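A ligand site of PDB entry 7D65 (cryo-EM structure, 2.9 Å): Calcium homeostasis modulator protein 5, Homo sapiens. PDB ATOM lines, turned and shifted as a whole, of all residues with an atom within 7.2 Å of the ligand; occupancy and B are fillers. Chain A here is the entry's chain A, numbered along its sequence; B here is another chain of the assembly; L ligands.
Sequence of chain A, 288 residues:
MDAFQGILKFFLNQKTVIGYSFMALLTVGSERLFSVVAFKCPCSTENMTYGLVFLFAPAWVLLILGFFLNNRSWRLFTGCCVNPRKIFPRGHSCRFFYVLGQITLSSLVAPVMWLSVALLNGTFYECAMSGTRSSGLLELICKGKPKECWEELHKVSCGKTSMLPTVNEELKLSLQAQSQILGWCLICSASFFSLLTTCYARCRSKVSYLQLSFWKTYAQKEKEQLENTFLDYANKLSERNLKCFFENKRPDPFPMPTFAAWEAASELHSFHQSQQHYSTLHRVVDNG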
ATOM      1  N   VAL A  28      13.805  16.869  -0.038  1.00  0.00           N
ATOM      2  CA  VAL A  28      14.785  15.829  -0.331  1.00  0.00           C
ATOM      3  C   VAL A  28      15.957  16.405  -1.106  1.00  0.00           C
ATOM      4  O   VAL A  28      17.124  16.197  -0.745  1.00  0.00           O
ATOM      5  CB  VAL A  28      14.107  14.665  -1.087  1.00  0.00           C
ATOM      6  CG1 VAL A  28      15.134  13.807  -1.804  1.00  0.00           C
ATOM      7  CG2 VAL A  28      13.300  13.816  -0.124  1.00  0.00           C
ATOM      8  N   GLU A  31      18.204  18.896   0.893  1.00  0.00           N
ATOM      9  CA  GLU A  31      19.073  18.289   1.895  1.00  0.00           C
ATOM     10  C   GLU A  31      20.351  17.754   1.271  1.00  0.00           C
ATOM     11  O   GLU A  31      21.406  17.783   1.908  1.00  0.00           O
ATOM     12  CB  GLU A  31      18.339  17.178   2.636  1.00  0.00           C
ATOM     13  CG  GLU A  31      18.977  16.775   3.951  1.00  0.00           C
ATOM     14  CD  GLU A  31      20.011  15.664   3.784  1.00  0.00           C
ATOM     15  OE1 GLU A  31      19.988  14.992   2.739  1.00  0.00           O
ATOM     16  OE2 GLU A  31      20.843  15.495   4.686  1.00  0.00           O
ATOM     17  N   ARG A  32      20.284  17.271   0.028  1.00  0.00           N
ATOM     18  CA  ARG A  32      21.482  16.796  -0.655  1.00  0.00           C
ATOM     19  C   ARG A  32      22.391  17.933  -1.073  1.00  0.00           C
ATOM     20  O   ARG A  32      23.574  17.703  -1.340  1.00  0.00           O
ATOM     21  CB  ARG A  32      21.085  15.970  -1.874  1.00  0.00           C
ATOM     22  CG  ARG A  32      20.341  14.691  -1.533  1.00  0.00           C
ATOM     23  CD  ARG A  32      21.164  13.787  -0.645  1.00  0.00           C
ATOM     24  NE  ARG A  32      22.301  13.231  -1.366  1.00  0.00           N
ATOM     25  CZ  ARG A  32      23.550  13.193  -0.899  1.00  0.00           C
ATOM     26  NH1 ARG A  32      23.828  13.678   0.295  1.00  0.00           N
ATOM     27  NH2 ARG A  32      24.510  12.664  -1.639  1.00  0.00           N
ATOM     28  N   SER A  35      24.407  18.534   2.665  1.00  0.00           N
ATOM     29  CA  SER A  35      25.294  17.505   3.199  1.00  0.00           C
ATOM     30  C   SER A  35      26.417  17.135   2.256  1.00  0.00           C
ATOM     31  O   SER A  35      27.339  16.412   2.661  1.00  0.00           O
ATOM     32  CB  SER A  35      24.502  16.260   3.555  1.00  0.00           C
ATOM     33  OG  SER A  35      24.025  15.614   2.389  1.00  0.00           O
ATOM     34  N   VAL A  36      26.378  17.588   1.010  1.00  0.00           N
ATOM     35  CA  VAL A  36      27.449  17.342   0.050  1.00  0.00           C
ATOM     36  C   VAL A  36      28.362  18.561  -0.074  1.00  0.00           C
ATOM     37  O   VAL A  36      29.587  18.429   0.002  1.00  0.00           O
ATOM     38  CB  VAL A  36      26.844  16.946  -1.323  1.00  0.00           C
ATOM     39  CG1 VAL A  36      27.825  17.196  -2.456  1.00  0.00           C
ATOM     40  CG2 VAL A  36      26.420  15.499  -1.305  1.00  0.00           C
ATOM     41  N   SER A 116      13.109  14.081   9.062  1.00  0.00           N
ATOM     42  CA  SER A 116      13.020  12.704   8.598  1.00  0.00           C
ATOM     43  C   SER A 116      14.014  12.429   7.475  1.00  0.00           C
ATOM     44  O   SER A 116      14.695  11.404   7.497  1.00  0.00           O
ATOM     45  CB  SER A 116      11.612  12.397   8.117  1.00  0.00           C
ATOM     46  OG  SER A 116      10.667  12.783   9.105  1.00  0.00           O
ATOM     47  N   VAL A 117      14.121  13.329   6.509  1.00  0.00           N
ATOM     48  CA  VAL A 117      15.063  13.156   5.413  1.00  0.00           C
ATOM     49  C   VAL A 117      16.489  13.377   5.888  1.00  0.00           C
ATOM     50  O   VAL A 117      17.426  12.736   5.384  1.00  0.00           O
ATOM     51  CB  VAL A 117      14.670  14.083   4.251  1.00  0.00           C
ATOM     52  CG1 VAL A 117      15.530  13.860   3.046  1.00  0.00           C
ATOM     53  CG2 VAL A 117      13.233  13.843   3.890  1.00  0.00           C
ATOM     54  N   ALA A 118      16.697  14.251   6.865  1.00  0.00           N
ATOM     55  CA  ALA A 118      18.049  14.507   7.337  1.00  0.00           C
ATOM     56  C   ALA A 118      18.565  13.415   8.259  1.00  0.00           C
ATOM     57  O   ALA A 118      19.783  13.285   8.396  1.00  0.00           O
ATOM     58  CB  ALA A 118      18.123  15.855   8.060  1.00  0.00           C
ATOM     59  N   LEU A 120      17.550  10.120   7.754  1.00  0.00           N
ATOM     60  CA  LEU A 120      17.679   8.978   6.875  1.00  0.00           C
ATOM     61  C   LEU A 120      18.913   9.051   5.984  1.00  0.00           C
ATOM     62  O   LEU A 120      19.236   8.070   5.315  1.00  0.00           O
ATOM     63  CB  LEU A 120      16.446   8.847   5.993  1.00  0.00           C
ATOM     64  CG  LEU A 120      15.186   8.226   6.584  1.00  0.00           C
ATOM     65  CD1 LEU A 120      14.037   8.455   5.644  1.00  0.00           C
ATOM     66  CD2 LEU A 120      15.386   6.761   6.819  1.00  0.00           C
ATOM     67  N   ASN A 121      19.561  10.196   5.934  1.00  0.00           N
ATOM     68  CA  ASN A 121      20.852  10.372   5.307  1.00  0.00           C
ATOM     69  C   ASN A 121      21.796  10.700   6.455  1.00  0.00           C
ATOM     70  O   ASN A 121      22.060  11.865   6.738  1.00  0.00           O
ATOM     71  CB  ASN A 121      20.793  11.483   4.275  1.00  0.00           C
ATOM     72  CG  ASN A 121      22.122  11.764   3.615  1.00  0.00           C
ATOM     73  OD1 ASN A 121      23.046  10.955   3.666  1.00  0.00           O
ATOM     74  ND2 ASN A 121      22.225  12.926   2.983  1.00  0.00           N
ATOM     75  N   GLY A 122      22.310   9.668   7.109  1.00  0.00           N
ATOM     76  CA  GLY A 122      22.857   9.838   8.440  1.00  0.00           C
ATOM     77  C   GLY A 122      24.204  10.508   8.595  1.00  0.00           C
ATOM     78  O   GLY A 122      25.046  10.017   9.349  1.00  0.00           O
ATOM     79  N   THR A 123      24.419  11.642   7.933  1.00  0.00           N
ATOM     80  CA  THR A 123      25.648  12.400   8.120  1.00  0.00           C
ATOM     81  C   THR A 123      25.563  13.364   9.291  1.00  0.00           C
ATOM     82  O   THR A 123      26.552  13.522  10.001  1.00  0.00           O
ATOM     83  CB  THR A 123      25.999  13.179   6.857  1.00  0.00           C
ATOM     84  OG1 THR A 123      25.132  14.304   6.734  1.00  0.00           O
ATOM     85  CG2 THR A 123      25.821  12.305   5.639  1.00  0.00           C
ATOM     86  N   GLN A 176      25.745   5.314  11.477  1.00  0.00           N
ATOM     87  CA  GLN A 176      24.936   5.684  10.329  1.00  0.00           C
ATOM     88  C   GLN A 176      23.671   4.842  10.236  1.00  0.00           C
ATOM     89  O   GLN A 176      22.744   5.229   9.524  1.00  0.00           O
ATOM     90  CB  GLN A 176      25.797   5.551   9.073  1.00  0.00           C
ATOM     91  CG  GLN A 176      25.294   6.188   7.789  1.00  0.00           C
ATOM     92  CD  GLN A 176      24.561   5.206   6.894  1.00  0.00           C
ATOM     93  OE1 GLN A 176      24.810   4.007   6.936  1.00  0.00           O
ATOM     94  NE2 GLN A 176      23.681   5.727   6.054  1.00  0.00           N
ATOM     95  N   GLN A 180      19.154   5.988  10.785  1.00  0.00           N
ATOM     96  CA  GLN A 180      18.126   5.553   9.856  1.00  0.00           C
ATOM     97  C   GLN A 180      17.030   4.765  10.550  1.00  0.00           C
ATOM     98  O   GLN A 180      15.967   4.585   9.968  1.00  0.00           O
ATOM     99  CB  GLN A 180      18.751   4.744   8.737  1.00  0.00           C
ATOM    100  CG  GLN A 180      19.609   5.568   7.831  1.00  0.00           C
ATOM    101  CD  GLN A 180      20.171   4.789   6.703  1.00  0.00           C
ATOM    102  OE1 GLN A 180      20.646   3.670   6.879  1.00  0.00           O
ATOM    103  NE2 GLN A 180      20.138   5.360   5.508  1.00  0.00           N
ATOM    104  N   TRP A 184      13.020   6.508  10.635  1.00  0.00           N
ATOM    105  CA  TRP A 184      11.764   5.818  10.340  1.00  0.00           C
ATOM    106  C   TRP A 184      10.810   5.797  11.516  1.00  0.00           C
ATOM    107  O   TRP A 184       9.616   5.596  11.319  1.00  0.00           O
ATOM    108  CB  TRP A 184      12.026   4.376   9.903  1.00  0.00           C
ATOM    109  CG  TRP A 184      12.519   4.217   8.501  1.00  0.00           C
ATOM    110  CD1 TRP A 184      13.697   3.682   8.120  1.00  0.00           C
ATOM    111  CD2 TRP A 184      11.828   4.555   7.294  1.00  0.00           C
ATOM    112  NE1 TRP A 184      13.815   3.687   6.768  1.00  0.00           N
ATOM    113  CE2 TRP A 184      12.669   4.208   6.222  1.00  0.00           C
ATOM    114  CE3 TRP A 184      10.585   5.118   7.010  1.00  0.00           C
ATOM    115  CZ2 TRP A 184      12.318   4.411   4.902  1.00  0.00           C
ATOM    116  CZ3 TRP A 184      10.240   5.317   5.701  1.00  0.00           C
ATOM    117  CH2 TRP A 184      11.104   4.970   4.667  1.00  0.00           C
ATOM    118  N   SER B  30      10.483   2.429  -6.705  1.00  0.00           N
ATOM    119  CA  SER B  30      10.820   3.084  -5.441  1.00  0.00           C
ATOM    120  C   SER B  30      11.589   2.172  -4.504  1.00  0.00           C
ATOM    121  O   SER B  30      12.301   2.678  -3.635  1.00  0.00           O
ATOM    122  CB  SER B  30       9.555   3.579  -4.736  1.00  0.00           C
ATOM    123  OG  SER B  30       9.861   4.083  -3.454  1.00  0.00           O
ATOM    124  N   LEU B  33      15.324   2.455  -5.354  1.00  0.00           N
ATOM    125  CA  LEU B  33      15.925   3.681  -4.843  1.00  0.00           C
ATOM    126  C   LEU B  33      16.356   3.539  -3.393  1.00  0.00           C
ATOM    127  O   LEU B  33      17.212   4.292  -2.940  1.00  0.00           O
ATOM    128  CB  LEU B  33      14.934   4.831  -5.012  1.00  0.00           C
ATOM    129  CG  LEU B  33      15.357   6.298  -4.887  1.00  0.00           C
ATOM    130  CD1 LEU B  33      14.594   7.120  -5.906  1.00  0.00           C
ATOM    131  CD2 LEU B  33      15.097   6.845  -3.497  1.00  0.00           C
ATOM    132  N   PHE B  34      15.779   2.585  -2.660  1.00  0.00           N
ATOM    133  CA  PHE B  34      16.107   2.392  -1.252  1.00  0.00           C
ATOM    134  C   PHE B  34      17.220   1.373  -1.055  1.00  0.00           C
ATOM    135  O   PHE B  34      18.144   1.615  -0.268  1.00  0.00           O
ATOM    136  CB  PHE B  34      14.868   1.969  -0.470  1.00  0.00           C
ATOM    137  CG  PHE B  34      14.057   3.104   0.044  1.00  0.00           C
ATOM    138  CD1 PHE B  34      14.448   3.790   1.183  1.00  0.00           C
ATOM    139  CD2 PHE B  34      12.897   3.500  -0.606  1.00  0.00           C
ATOM    140  CE1 PHE B  34      13.692   4.845   1.658  1.00  0.00           C
ATOM    141  CE2 PHE B  34      12.141   4.554  -0.131  1.00  0.00           C
ATOM    142  CZ  PHE B  34      12.539   5.227   1.001  1.00  0.00           C
ATOM    143  N   VAL B  36      19.578   0.448  -2.996  1.00  0.00           N
ATOM    144  CA  VAL B  36      20.835   0.806  -3.641  1.00  0.00           C
ATOM    145  C   VAL B  36      21.485   2.006  -2.959  1.00  0.00           C
ATOM    146  O   VAL B  36      22.667   1.979  -2.625  1.00  0.00           O
ATOM    147  CB  VAL B  36      20.594   1.069  -5.148  1.00  0.00           C
ATOM    148  CG1 VAL B  36      21.693   1.921  -5.754  1.00  0.00           C
ATOM    149  CG2 VAL B  36      20.474  -0.246  -5.897  1.00  0.00           C
ATOM    150  N   VAL B  37      20.700   3.044  -2.708  1.00  0.00           N
ATOM    151  CA  VAL B  37      21.227   4.327  -2.275  1.00  0.00           C
ATOM    152  C   VAL B  37      21.270   4.454  -0.760  1.00  0.00           C
ATOM    153  O   VAL B  37      22.221   4.996  -0.195  1.00  0.00           O
ATOM    154  CB  VAL B  37      20.399   5.451  -2.928  1.00  0.00           C
ATOM    155  CG1 VAL B  37      21.062   6.772  -2.724  1.00  0.00           C
ATOM    156  CG2 VAL B  37      20.241   5.178  -4.406  1.00  0.00           C
ATOM    157  N   ALA B  38      20.248   3.952  -0.057  1.00  0.00           N
ATOM    158  CA  ALA B  38      20.133   4.176   1.375  1.00  0.00           C
ATOM    159  C   ALA B  38      20.455   2.966   2.228  1.00  0.00           C
ATOM    160  O   ALA B  38      20.957   3.137   3.338  1.00  0.00           O
ATOM    161  CB  ALA B  38      18.713   4.659   1.718  1.00  0.00           C
ATOM    162  N   PHE B  39      20.174   1.745   1.769  1.00  0.00           N
ATOM    163  CA  PHE B  39      20.376   0.558   2.598  1.00  0.00           C
ATOM    164  C   PHE B  39      21.822   0.115   2.527  1.00  0.00           C
ATOM    165  O   PHE B  39      22.336  -0.179   1.437  1.00  0.00           O
ATOM    166  CB  PHE B  39      19.449  -0.570   2.136  1.00  0.00           C
ATOM    167  CG  PHE B  39      19.414  -1.746   3.079  1.00  0.00           C
ATOM    168  CD1 PHE B  39      20.201  -2.852   2.867  1.00  0.00           C
ATOM    169  CD2 PHE B  39      18.554  -1.755   4.154  1.00  0.00           C
ATOM    170  CE1 PHE B  39      20.154  -3.922   3.711  1.00  0.00           C
ATOM    171  CE2 PHE B  39      18.512  -2.839   5.001  1.00  0.00           C
ATOM    172  CZ  PHE B  39      19.316  -3.908   4.789  1.00  0.00           C
ATOM    173  N   LYS B  40      22.484   0.067   3.674  1.00  0.00           N
ATOM    174  CA  LYS B  40      23.764  -0.633   3.817  1.00  0.00           C
ATOM    175  C   LYS B  40      23.793  -1.270   5.184  1.00  0.00           C
ATOM    176  O   LYS B  40      23.757  -0.570   6.199  1.00  0.00           O
ATOM    177  CB  LYS B  40      24.968   0.297   3.614  1.00  0.00           C
ATOM    178  CG  LYS B  40      24.753   1.729   4.033  1.00  0.00           C
ATOM    179  CD  LYS B  40      26.015   2.532   3.818  1.00  0.00           C
ATOM    180  CE  LYS B  40      26.399   2.558   2.346  1.00  0.00           C
ATOM    181  NZ  LYS B  40      25.454   3.330   1.503  1.00  0.00           N
HETATM  182  O1  LIG L   1      24.537   7.243   0.964  1.00  0.00           O
HETATM  183  O2  LIG L   1      23.202   7.490   3.020  1.00  0.00           O
HETATM  184  P1  LIG L   1      23.900   8.226   1.905  1.00  0.00           P
HETATM  185  O3  LIG L   1      24.970   9.109   2.494  1.00  0.00           O
HETATM  186  O4  LIG L   1      22.797   9.138   1.078  1.00  0.00           O
HETATM  187  C1  LIG L   1      21.433   8.869   1.249  1.00  0.00           C
HETATM  188  C2  LIG L   1      20.636   9.334   0.021  1.00  0.00           C
HETATM  189  C3  LIG L   1      19.280   9.830   0.504  1.00  0.00           C
HETATM  190  O5  LIG L   1      18.281   8.910   0.146  1.00  0.00           O
HETATM  191  C4  LIG L   1      17.019   9.229   0.653  1.00  0.00           C
HETATM  192  O6  LIG L   1      16.915   9.607   1.769  1.00  0.00           O
HETATM  193  C5  LIG L   1      15.762   9.088  -0.202  1.00  0.00           C
HETATM  194  C6  LIG L   1      14.567   9.816   0.412  1.00  0.00           C
HETATM  195  C7  LIG L   1      13.265   9.025   0.294  1.00  0.00           C
HETATM  196  O7  LIG L   1      21.297  10.380  -0.659  1.00  0.00           O
HETATM  197  C8  LIG L   1      21.988  10.038  -1.834  1.00  0.00           C
HETATM  198  O8  LIG L   1      22.965   9.370  -1.774  1.00  0.00           O
HETATM  199  C9  LIG L   1      21.530  10.512  -3.212  1.00  0.00           C
HETATM  200  C10 LIG L   1      20.027  10.423  -3.462  1.00  0.00           C
HETATM  201  C11 LIG L   1      19.693  10.553  -4.947  1.00  0.00           C
HETATM  202  C12 LIG L   1      18.215  10.839  -5.190  1.00  0.00           C
HETATM  203  C13 LIG L   1      17.849  10.774  -6.682  1.00  0.00           C
HETATM  204  C14 LIG L   1      16.345  10.885  -6.923  1.00  0.00           C
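The side-chain amide oxygen (OD1) of Asn 121 lies close to an oxygen (O3) of the ligand, 2.9 Å away.
O7 of the ligand sits at hydrogen-bond distance from NE of Arg 32 (3.1 Å).
The backbone carbonyl oxygen (O) of Val 37 of chain B lies close to an oxygen (O1) of the ligand.
Gln 176 touches the ligand.
CZ of Phe 34 of chain B touches C7 of the ligand, at 3.9 Å.
Hydrophobic or aromatic side chains that line the ligand: Phe 34 of chain B and Val 37 of chain B.
Five residues have an atom within 4 Å of the ligand: Arg 32, Asn 121, Gln 176, Phe 34 of chain B and Val 37 of chain B.
The nearest printed residue that does not touch the ligand is Leu 33 of chain B (4.04 Å).
The side-chain amide nitrogen (ND2) of Asn 121 sits close to the guanidinium group (NH1) of Arg 32 (3.2 Å).
The side-chain carboxylate of Glu 31 sits at hydrogen-bond distance from the side-chain amide nitrogen of Asn 121, 3.1 Å away.
The side-chain hydroxyl (OG) of Ser 35 lies within hydrogen-bond range of the side-chain amide nitrogen (ND2) of Asn 121, at 3.3 Å.
The guanidinium group (NH1) of Arg 32 lies within hydrogen-bond range of the side-chain hydroxyl (OG) of Ser 35.
The backbone carbonyl oxygen (O) of Phe 34 of chain B is in hydrogen-bond range of the backbone NH (N) of Phe 39 of chain B, at 2.9 Å.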
